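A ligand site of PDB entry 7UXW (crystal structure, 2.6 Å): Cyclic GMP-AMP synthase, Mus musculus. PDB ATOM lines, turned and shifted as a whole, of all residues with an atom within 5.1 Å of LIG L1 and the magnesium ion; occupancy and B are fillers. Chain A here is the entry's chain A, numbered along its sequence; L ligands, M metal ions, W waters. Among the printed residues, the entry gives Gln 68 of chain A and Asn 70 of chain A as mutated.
NE2 of Gln 68 is in hydrogen-bond range of OD2 of Asp 164. The backbone NH (N) of Thr 54 lies within hydrogen-bond range of the backbone carbonyl oxygen (O) of Asn 70 (3.0 Å). OG of Ser 223 lies within hydrogen-bond range of OG of Ser 225. The backbone NH (N) of Asp 164 is in hydrogen-bond range of the backbone carbonyl oxygen (O) of Phe 69 (3.1 Å). The backbone carbonyl oxygen (O) of Arg 221 lies within hydrogen-bond range of the backbone NH (N) of Val 205 (2.7 Å). The backbone NH (N) of Ala 150 is in hydrogen-bond range of the side-chain hydroxyl (OG) of Ser 148 (3.3 Å).
Water W1 bridges the backbone carbonyl oxygen of Gln 68 (3.1 Å) and the backbone NH of Ser 56 (3.5 Å).
Gly 147 touches LIG L1 (C to O6, 3.7 Å). CG of Pro 149 touches C6 of LIG L1, at 3.6 Å. Ala 150 touches LIG L1. Ile 166 touches LIG L1. Hydrophobic or aromatic side chains that line LIG L1: Met 72, Pro 149, Ala 150 and Ile 166. 15 residues have an atom within 4 Å of LIG L1: Thr 54, Gln 68, Asn 70, Met 72, Lys 145, Gly 147, Ser 148, Pro 149, Ala 150, Asp 164, Ile 166, Lys 207, Arg 221, Ser 223 and Ser 225. The nearest printed residue that does not touch LIG L1 is Val 205 (4.1 Å).
The side-chain amide nitrogen (ND2) of Asn 70 sits at hydrogen-bond distance from an oxygen (O13) of LIG L1. The side-chain hydroxyl of Ser 223 lies within hydrogen-bond range of an oxygen (O14) of LIG L1, 2.5 Å away. OD2 of Asp 164 lies within hydrogen-bond range of O13 of LIG L1, at 2.6 Å. O5 of LIG L1 lies within salt-bridge range of NZ of Lys 145. An oxygen (O8) of LIG L1 lies within salt-bridge range of the guanidinium group (NH1) of Arg 221, 3.0 Å away. The side-chain hydroxyl of Ser 225 lies within hydrogen-bond range of a nitrogen (N3) of LIG L1 (2.9 Å). N4 of LIG L1 is in hydrogen-bond range of OG1 of Thr 54, at 2.9 Å. N of Ser 148 sits close to O6 of LIG L1 (3.4 Å). A nitrogen (N4) of LIG L1 sits close to the side-chain sulfur (SD) of Met 72. The side-chain amino group (NZ) of Lys 207 lies within salt-bridge range of an oxygen (O6) of LIG L1 (3.8 Å). OG of Ser 225 is in hydrogen-bond range of O13 of LG2 L2, at 2.7 Å. An oxygen (O5) of LG2 L2 lies close to the backbone NH (N) of Ser 56, at 2.9 Å. OG of Ser 56 lies within hydrogen-bond range of O1 of LG2 L2, 2.6 Å away.
An oxygen (O12) of LIG L1 sits at hydrogen-bond distance from an oxygen (O7) of LG2 L2 (2.7 Å).
The magnesium ion is bound by an oxygen (O2) of LG2 L2 (2.0 Å), water W1 (2.1 Å), the side-chain amide oxygen (OE1) of Gln 68 (2.1 Å), an oxygen (O5) of LG2 L2 (2.1 Å), an oxygen (O8) of LG2 L2 (2.1 Å) and the side-chain amide oxygen (OD1) of Asn 70 (2.2 Å). The magnesium ion has six donor atoms within binding distance.
OG of Ser 56 touches the magnesium ion (3.5 Å). Of the 23 residues printed, 3 come within 4 Å of the magnesium ion. Along chain A the residues within 4 Å of the magnesium ion span positions 56 to 70. The nearest printed residue that does not touch the magnesium ion is Gly 55 (4.8 Å).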
ATOM      1  N   THR A  54      26.799  -2.715  18.141  1.00  0.00           N
ATOM      2  CA  THR A  54      25.791  -1.699  17.917  1.00  0.00           C
ATOM      3  C   THR A  54      24.742  -1.630  19.030  1.00  0.00           C
ATOM      4  O   THR A  54      24.783  -2.395  20.009  1.00  0.00           O
ATOM      5  CB  THR A  54      25.114  -1.959  16.568  1.00  0.00           C
ATOM      6  OG1 THR A  54      24.700  -3.329  16.512  1.00  0.00           O
ATOM      7  CG2 THR A  54      26.071  -1.692  15.458  1.00  0.00           C
ATOM      8  N   GLY A  55      23.835  -0.668  18.875  1.00  0.00           N
ATOM      9  CA  GLY A  55      22.715  -0.503  19.777  1.00  0.00           C
ATOM     10  C   GLY A  55      23.088   0.186  21.068  1.00  0.00           C
ATOM     11  O   GLY A  55      24.190   0.730  21.194  1.00  0.00           O
ATOM     12  N   SER A  56      22.173   0.100  22.041  1.00  0.00           N
ATOM     13  CA  SER A  56      22.138   1.010  23.175  1.00  0.00           C
ATOM     14  C   SER A  56      23.357   0.867  24.067  1.00  0.00           C
ATOM     15  O   SER A  56      23.886   1.866  24.543  1.00  0.00           O
ATOM     16  CB  SER A  56      20.832   0.867  23.987  1.00  0.00           C
ATOM     17  OG  SER A  56      20.544  -0.481  24.362  1.00  0.00           O
ATOM     18  N   GLN A  68      20.883  -6.518  27.544  1.00  0.00           N
ATOM     19  CA  GLN A  68      20.628  -6.692  26.139  1.00  0.00           C
ATOM     20  C   GLN A  68      21.760  -6.032  25.354  1.00  0.00           C
ATOM     21  O   GLN A  68      22.081  -4.879  25.604  1.00  0.00           O
ATOM     22  CB  GLN A  68      19.238  -6.142  25.778  1.00  0.00           C
ATOM     23  CG  GLN A  68      18.631  -6.787  24.538  1.00  0.00           C
ATOM     24  CD  GLN A  68      18.866  -5.982  23.271  1.00  0.00           C
ATOM     25  OE1 GLN A  68      19.640  -5.044  23.235  1.00  0.00           O
ATOM     26  NE2 GLN A  68      18.167  -6.342  22.209  1.00  0.00           N
ATOM     27  N   PHE A  69      22.383  -6.819  24.465  1.00  0.00           N
ATOM     28  CA  PHE A  69      23.531  -6.412  23.653  1.00  0.00           C
ATOM     29  C   PHE A  69      23.219  -6.700  22.189  1.00  0.00           C
ATOM     30  O   PHE A  69      22.666  -7.744  21.868  1.00  0.00           O
ATOM     31  CB  PHE A  69      24.776  -7.235  24.022  1.00  0.00           C
ATOM     32  CG  PHE A  69      25.301  -6.958  25.397  1.00  0.00           C
ATOM     33  CD1 PHE A  69      24.681  -7.524  26.520  1.00  0.00           C
ATOM     34  CD2 PHE A  69      26.421  -6.166  25.574  1.00  0.00           C
ATOM     35  CE1 PHE A  69      25.171  -7.289  27.794  1.00  0.00           C
ATOM     36  CE2 PHE A  69      26.901  -5.902  26.853  1.00  0.00           C
ATOM     37  CZ  PHE A  69      26.280  -6.472  27.959  1.00  0.00           C
ATOM     38  N   ASN A  70      23.636  -5.794  21.306  1.00  0.00           N
ATOM     39  CA  ASN A  70      23.454  -5.985  19.866  1.00  0.00           C
ATOM     40  C   ASN A  70      24.789  -6.083  19.136  1.00  0.00           C
ATOM     41  O   ASN A  70      25.661  -5.249  19.330  1.00  0.00           O
ATOM     42  CB  ASN A  70      22.600  -4.865  19.295  1.00  0.00           C
ATOM     43  CG  ASN A  70      21.303  -4.680  20.068  1.00  0.00           C
ATOM     44  OD1 ASN A  70      21.233  -3.907  21.016  1.00  0.00           O
ATOM     45  ND2 ASN A  70      20.247  -5.363  19.629  1.00  0.00           N
ATOM     46  N   MET A  72      26.448  -7.126  15.145  1.00  0.00           N
ATOM     47  CA  MET A  72      26.311  -7.465  13.746  1.00  0.00           C
ATOM     48  C   MET A  72      27.527  -8.279  13.323  1.00  0.00           C
ATOM     49  O   MET A  72      28.665  -7.915  13.593  1.00  0.00           O
ATOM     50  CB  MET A  72      26.143  -6.200  12.880  1.00  0.00           C
ATOM     51  CG  MET A  72      24.866  -5.445  13.232  1.00  0.00           C
ATOM     52  SD  MET A  72      24.621  -3.855  12.407  1.00  0.00           S
ATOM     53  CE  MET A  72      24.383  -4.407  10.708  1.00  0.00           C
ATOM     54  N   LYS A 145      11.727 -16.178  16.353  1.00  0.00           N
ATOM     55  CA  LYS A 145      10.527 -15.378  16.172  1.00  0.00           C
ATOM     56  C   LYS A 145      10.425 -15.108  14.681  1.00  0.00           C
ATOM     57  O   LYS A 145      11.322 -14.479  14.115  1.00  0.00           O
ATOM     58  CB  LYS A 145      10.618 -14.073  16.971  1.00  0.00           C
ATOM     59  CG  LYS A 145       9.281 -13.666  17.589  1.00  0.00           C
ATOM     60  CD  LYS A 145       9.133 -12.155  17.667  1.00  0.00           C
ATOM     61  CE  LYS A 145       8.868 -11.562  16.299  1.00  0.00           C
ATOM     62  NZ  LYS A 145       8.659 -10.095  16.396  1.00  0.00           N
ATOM     63  N   PRO A 146       9.365 -15.574  13.993  1.00  0.00           N
ATOM     64  CA  PRO A 146       9.270 -15.484  12.540  1.00  0.00           C
ATOM     65  C   PRO A 146       9.450 -14.038  12.032  1.00  0.00           C
ATOM     66  O   PRO A 146       9.096 -13.126  12.749  1.00  0.00           O
ATOM     67  CB  PRO A 146       7.872 -15.995  12.203  1.00  0.00           C
ATOM     68  CG  PRO A 146       7.485 -16.868  13.392  1.00  0.00           C
ATOM     69  CD  PRO A 146       8.181 -16.227  14.587  1.00  0.00           C
ATOM     70  N   GLY A 147      10.020 -13.889  10.836  1.00  0.00           N
ATOM     71  CA  GLY A 147      10.267 -12.585  10.236  1.00  0.00           C
ATOM     72  C   GLY A 147      11.493 -11.828  10.739  1.00  0.00           C
ATOM     73  O   GLY A 147      12.048 -11.026   9.983  1.00  0.00           O
ATOM     74  N   SER A 148      11.910 -12.101  11.992  1.00  0.00           N
ATOM     75  CA  SER A 148      13.028 -11.412  12.677  1.00  0.00           C
ATOM     76  C   SER A 148      14.399 -11.742  12.092  1.00  0.00           C
ATOM     77  O   SER A 148      14.676 -12.881  11.702  1.00  0.00           O
ATOM     78  CB  SER A 148      13.029 -11.745  14.182  1.00  0.00           C
ATOM     79  OG  SER A 148      14.122 -11.160  14.869  1.00  0.00           O
ATOM     80  N   PRO A 149      15.324 -10.759  12.009  1.00  0.00           N
ATOM     81  CA  PRO A 149      16.668 -11.002  11.493  1.00  0.00           C
ATOM     82  C   PRO A 149      17.633 -11.539  12.558  1.00  0.00           C
ATOM     83  O   PRO A 149      18.758 -11.900  12.228  1.00  0.00           O
ATOM     84  CB  PRO A 149      17.083  -9.599  11.028  1.00  0.00           C
ATOM     85  CG  PRO A 149      16.429  -8.673  12.051  1.00  0.00           C
ATOM     86  CD  PRO A 149      15.115  -9.359  12.403  1.00  0.00           C
ATOM     87  N   ALA A 150      17.176 -11.569  13.815  1.00  0.00           N
ATOM     88  CA  ALA A 150      18.046 -11.851  14.940  1.00  0.00           C
ATOM     89  C   ALA A 150      18.189 -13.338  15.171  1.00  0.00           C
ATOM     90  O   ALA A 150      17.271 -14.098  14.907  1.00  0.00           O
ATOM     91  CB  ALA A 150      17.500 -11.173  16.193  1.00  0.00           C
ATOM     92  N   ASP A 164      21.418 -10.307  20.759  1.00  0.00           N
ATOM     93  CA  ASP A 164      20.878 -10.460  19.419  1.00  0.00           C
ATOM     94  C   ASP A 164      22.032 -10.400  18.437  1.00  0.00           C
ATOM     95  O   ASP A 164      22.621  -9.347  18.249  1.00  0.00           O
ATOM     96  CB  ASP A 164      19.879  -9.354  19.107  1.00  0.00           C
ATOM     97  CG  ASP A 164      18.542  -9.529  19.828  1.00  0.00           C
ATOM     98  OD1 ASP A 164      18.346 -10.551  20.493  1.00  0.00           O
ATOM     99  OD2 ASP A 164      17.688  -8.634  19.711  1.00  0.00           O
ATOM    100  N   ILE A 166      23.110 -10.390  14.797  1.00  0.00           N
ATOM    101  CA  ILE A 166      22.448  -9.987  13.563  1.00  0.00           C
ATOM    102  C   ILE A 166      23.358 -10.199  12.360  1.00  0.00           C
ATOM    103  O   ILE A 166      24.420  -9.606  12.279  1.00  0.00           O
ATOM    104  CB  ILE A 166      22.015  -8.516  13.632  1.00  0.00           C
ATOM    105  CG1 ILE A 166      20.869  -8.352  14.655  1.00  0.00           C
ATOM    106  CG2 ILE A 166      21.592  -7.991  12.275  1.00  0.00           C
ATOM    107  CD1 ILE A 166      21.307  -7.736  15.985  1.00  0.00           C
ATOM    108  N   VAL A 205      19.913  -6.489   6.369  1.00  0.00           N
ATOM    109  CA  VAL A 205      19.704  -7.558   7.326  1.00  0.00           C
ATOM    110  C   VAL A 205      18.511  -8.400   6.878  1.00  0.00           C
ATOM    111  O   VAL A 205      17.615  -7.901   6.201  1.00  0.00           O
ATOM    112  CB  VAL A 205      19.472  -7.015   8.760  1.00  0.00           C
ATOM    113  CG1 VAL A 205      20.694  -6.226   9.219  1.00  0.00           C
ATOM    114  CG2 VAL A 205      18.212  -6.181   8.859  1.00  0.00           C
ATOM    115  N   LYS A 207      15.392  -9.356   7.326  1.00  0.00           N
ATOM    116  CA  LYS A 207      14.098  -9.109   7.935  1.00  0.00           C
ATOM    117  C   LYS A 207      13.150  -9.150   6.768  1.00  0.00           C
ATOM    118  O   LYS A 207      13.413  -8.491   5.761  1.00  0.00           O
ATOM    119  CB  LYS A 207      14.063  -7.715   8.573  1.00  0.00           C
ATOM    120  CG  LYS A 207      12.678  -7.190   8.914  1.00  0.00           C
ATOM    121  CD  LYS A 207      12.293  -7.453  10.357  1.00  0.00           C
ATOM    122  CE  LYS A 207      10.857  -7.027  10.641  1.00  0.00           C
ATOM    123  NZ  LYS A 207       9.854  -7.807   9.844  1.00  0.00           N
ATOM    124  N   ARG A 221      16.279  -5.895   4.697  1.00  0.00           N
ATOM    125  CA  ARG A 221      15.988  -4.519   5.196  1.00  0.00           C
ATOM    126  C   ARG A 221      17.302  -3.776   5.407  1.00  0.00           C
ATOM    127  O   ARG A 221      18.273  -4.414   5.878  1.00  0.00           O
ATOM    128  CB  ARG A 221      15.196  -4.554   6.515  1.00  0.00           C
ATOM    129  CG  ARG A 221      14.636  -3.207   6.954  1.00  0.00           C
ATOM    130  CD  ARG A 221      13.796  -3.303   8.218  1.00  0.00           C
ATOM    131  NE  ARG A 221      14.614  -3.568   9.401  1.00  0.00           N
ATOM    132  CZ  ARG A 221      14.154  -3.984  10.575  1.00  0.00           C
ATOM    133  NH1 ARG A 221      12.864  -4.196  10.767  1.00  0.00           N
ATOM    134  NH2 ARG A 221      15.000  -4.203  11.578  1.00  0.00           N
ATOM    135  N   LEU A 222      17.335  -2.476   5.096  1.00  0.00           N
ATOM    136  CA  LEU A 222      18.526  -1.655   5.340  1.00  0.00           C
ATOM    137  C   LEU A 222      18.781  -1.517   6.838  1.00  0.00           C
ATOM    138  O   LEU A 222      17.847  -1.424   7.619  1.00  0.00           O
ATOM    139  CB  LEU A 222      18.388  -0.258   4.708  1.00  0.00           C
ATOM    140  CG  LEU A 222      18.407  -0.233   3.190  1.00  0.00           C
ATOM    141  CD1 LEU A 222      17.926   1.083   2.639  1.00  0.00           C
ATOM    142  CD2 LEU A 222      19.814  -0.538   2.692  1.00  0.00           C
ATOM    143  N   SER A 223      20.059  -1.504   7.207  1.00  0.00           N
ATOM    144  CA  SER A 223      20.489  -1.121   8.542  1.00  0.00           C
ATOM    145  C   SER A 223      21.505   0.027   8.480  1.00  0.00           C
ATOM    146  O   SER A 223      22.413   0.036   7.645  1.00  0.00           O
ATOM    147  CB  SER A 223      21.114  -2.305   9.257  1.00  0.00           C
ATOM    148  OG  SER A 223      21.461  -1.915  10.587  1.00  0.00           O
ATOM    149  N   PHE A 224      21.327   0.996   9.396  1.00  0.00           N
ATOM    150  CA  PHE A 224      22.206   2.142   9.578  1.00  0.00           C
ATOM    151  C   PHE A 224      22.687   2.224  11.039  1.00  0.00           C
ATOM    152  O   PHE A 224      22.916   3.325  11.555  1.00  0.00           O
ATOM    153  CB  PHE A 224      21.441   3.416   9.192  1.00  0.00           C
ATOM    154  CG  PHE A 224      20.991   3.391   7.775  1.00  0.00           C
ATOM    155  CD1 PHE A 224      21.915   3.601   6.741  1.00  0.00           C
ATOM    156  CD2 PHE A 224      19.686   3.097   7.458  1.00  0.00           C
ATOM    157  CE1 PHE A 224      21.516   3.571   5.436  1.00  0.00           C
ATOM    158  CE2 PHE A 224      19.271   3.050   6.147  1.00  0.00           C
ATOM    159  CZ  PHE A 224      20.186   3.294   5.134  1.00  0.00           C
ATOM    160  N   SER A 225      22.840   1.056  11.679  1.00  0.00           N
ATOM    161  CA  SER A 225      23.207   0.968  13.079  1.00  0.00           C
ATOM    162  C   SER A 225      24.567   1.555  13.351  1.00  0.00           C
ATOM    163  O   SER A 225      24.811   2.099  14.421  1.00  0.00           O
ATOM    164  CB  SER A 225      23.196  -0.492  13.530  1.00  0.00           C
ATOM    165  OG  SER A 225      21.870  -0.938  13.674  1.00  0.00           O
ATOM    166  N   CYS A 276       8.321  -0.111  19.808  1.00  0.00           N
ATOM    167  CA  CYS A 276       9.659  -0.554  20.175  1.00  0.00           C
ATOM    168  C   CYS A 276      10.567   0.636  20.351  1.00  0.00           C
ATOM    169  O   CYS A 276      10.187   1.760  20.058  1.00  0.00           O
ATOM    170  CB  CYS A 276      10.224  -1.492  19.105  1.00  0.00           C
ATOM    171  SG  CYS A 276      10.473  -0.680  17.502  1.00  0.00           S
HETATM  172  P1  LIG L   1       9.073  -6.079  15.357  1.00  0.00           P
HETATM  173  O1  LIG L   1       9.579  -6.495  16.714  1.00  0.00           O
HETATM  174  O2  LIG L   1       9.625  -4.749  14.911  1.00  0.00           O
HETATM  175  O3  LIG L   1       7.567  -6.150  15.243  1.00  0.00           O
HETATM  176  O4  LIG L   1       9.624  -7.164  14.289  1.00  0.00           O
HETATM  177  P2  LIG L   1      10.781  -8.275  14.346  1.00  0.00           P
HETATM  178  O5  LIG L   1      10.952  -8.710  15.768  1.00  0.00           O
HETATM  179  O6  LIG L   1      10.549  -9.292  13.279  1.00  0.00           O
HETATM  180  O7  LIG L   1      12.055  -7.403  13.931  1.00  0.00           O
HETATM  181  P3  LIG L   1      12.779  -6.150  14.634  1.00  0.00           P
HETATM  182  O8  LIG L   1      12.907  -5.063  13.629  1.00  0.00           O
HETATM  183  O9  LIG L   1      12.093  -5.847  15.925  1.00  0.00           O
HETATM  184  O10 LIG L   1      14.217  -6.792  14.933  1.00  0.00           O
HETATM  185  C1  LIG L   1      14.380  -7.634  16.094  1.00  0.00           C
HETATM  186  C2  LIG L   1      15.691  -7.320  16.762  1.00  0.00           C
HETATM  187  O11 LIG L   1      16.769  -7.596  15.836  1.00  0.00           O
HETATM  188  C3  LIG L   1      15.917  -5.859  17.166  1.00  0.00           C
HETATM  189  O12 LIG L   1      15.313  -5.524  18.410  1.00  0.00           O
HETATM  190  C4  LIG L   1      17.443  -5.819  17.239  1.00  0.00           C
HETATM  191  O13 LIG L   1      17.966  -6.394  18.414  1.00  0.00           O
HETATM  192  C5  LIG L   1      17.799  -6.647  16.001  1.00  0.00           C
HETATM  193  N1  LIG L   1      17.923  -5.835  14.796  1.00  0.00           N
HETATM  194  C6  LIG L   1      16.969  -5.623  13.834  1.00  0.00           C
HETATM  195  N2  LIG L   1      17.374  -4.841  12.863  1.00  0.00           N
HETATM  196  C7  LIG L   1      18.678  -4.507  13.224  1.00  0.00           C
HETATM  197  C8  LIG L   1      19.622  -3.678  12.565  1.00  0.00           C
HETATM  198  O14 LIG L   1      19.467  -3.050  11.511  1.00  0.00           O
HETATM  199  N3  LIG L   1      20.824  -3.605  13.268  1.00  0.00           N
HETATM  200  C9  LIG L   1      21.090  -4.243  14.457  1.00  0.00           C
HETATM  201  N4  LIG L   1      22.299  -4.051  14.987  1.00  0.00           N
HETATM  202  N5  LIG L   1      20.203  -5.024  15.083  1.00  0.00           N
HETATM  203  C10 LIG L   1      19.023  -5.110  14.407  1.00  0.00           C
HETATM  204  P1  LG2 L   2      17.443  -1.180  23.615  1.00  0.00           P
HETATM  205  O1  LG2 L   2      18.023  -0.590  24.880  1.00  0.00           O
HETATM  206  O2  LG2 L   2      18.049  -2.524  23.292  1.00  0.00           O
HETATM  207  O3  LG2 L   2      15.932  -1.192  23.623  1.00  0.00           O
HETATM  208  P2  LG2 L   2      18.587  -0.495  21.014  1.00  0.00           P
HETATM  209  O4  LG2 L   2      18.752   0.777  20.246  1.00  0.00           O
HETATM  210  O5  LG2 L   2      19.786  -1.331  21.287  1.00  0.00           O
HETATM  211  O6  LG2 L   2      17.845  -0.196  22.397  1.00  0.00           O
HETATM  212  P3  LG2 L   2      17.398  -2.886  19.783  1.00  0.00           P
HETATM  213  O7  LG2 L   2      15.962  -3.262  19.652  1.00  0.00           O
HETATM  214  O8  LG2 L   2      18.294  -3.680  20.688  1.00  0.00           O
HETATM  215  O9  LG2 L   2      17.471  -1.368  20.297  1.00  0.00           O
HETATM  216  O10 LG2 L   2      18.015  -2.803  18.304  1.00  0.00           O
HETATM  217  C1  LG2 L   2      19.428  -2.636  18.064  1.00  0.00           C
HETATM  218  C2  LG2 L   2      19.636  -1.708  16.892  1.00  0.00           C
HETATM  219  O11 LG2 L   2      19.037  -2.277  15.687  1.00  0.00           O
HETATM  220  C3  LG2 L   2      18.981  -0.322  16.986  1.00  0.00           C
HETATM  221  O12 LG2 L   2      19.763   0.569  17.770  1.00  0.00           O
HETATM  222  C4  LG2 L   2      18.924   0.079  15.508  1.00  0.00           C
HETATM  223  O13 LG2 L   2      20.159   0.578  15.044  1.00  0.00           O
HETATM  224  C5  LG2 L   2      18.560  -1.250  14.851  1.00  0.00           C
HETATM  225  N1  LG2 L   2      17.107  -1.438  14.657  1.00  0.00           N
HETATM  226  C6  LG2 L   2      16.209  -1.964  15.554  1.00  0.00           C
HETATM  227  N2  LG2 L   2      14.975  -1.985  15.078  1.00  0.00           N
HETATM  228  C7  LG2 L   2      15.083  -1.433  13.800  1.00  0.00           C
HETATM  229  C8  LG2 L   2      14.137  -1.180  12.792  1.00  0.00           C
HETATM  230  N3  LG2 L   2      12.846  -1.454  12.911  1.00  0.00           N
HETATM  231  N4  LG2 L   2      14.583  -0.621  11.643  1.00  0.00           N
HETATM  232  C9  LG2 L   2      15.895  -0.351  11.531  1.00  0.00           C
HETATM  233  N5  LG2 L   2      16.871  -0.546  12.410  1.00  0.00           N
HETATM  234  C10 LG2 L   2      16.398  -1.097  13.541  1.00  0.00           C
HETATM  235 MG    MG M   1      19.640  -3.188  22.281  1.00  0.00          MG
HETATM  236  O   HOH W   1      21.029  -2.694  23.748  1.00  0.00           O
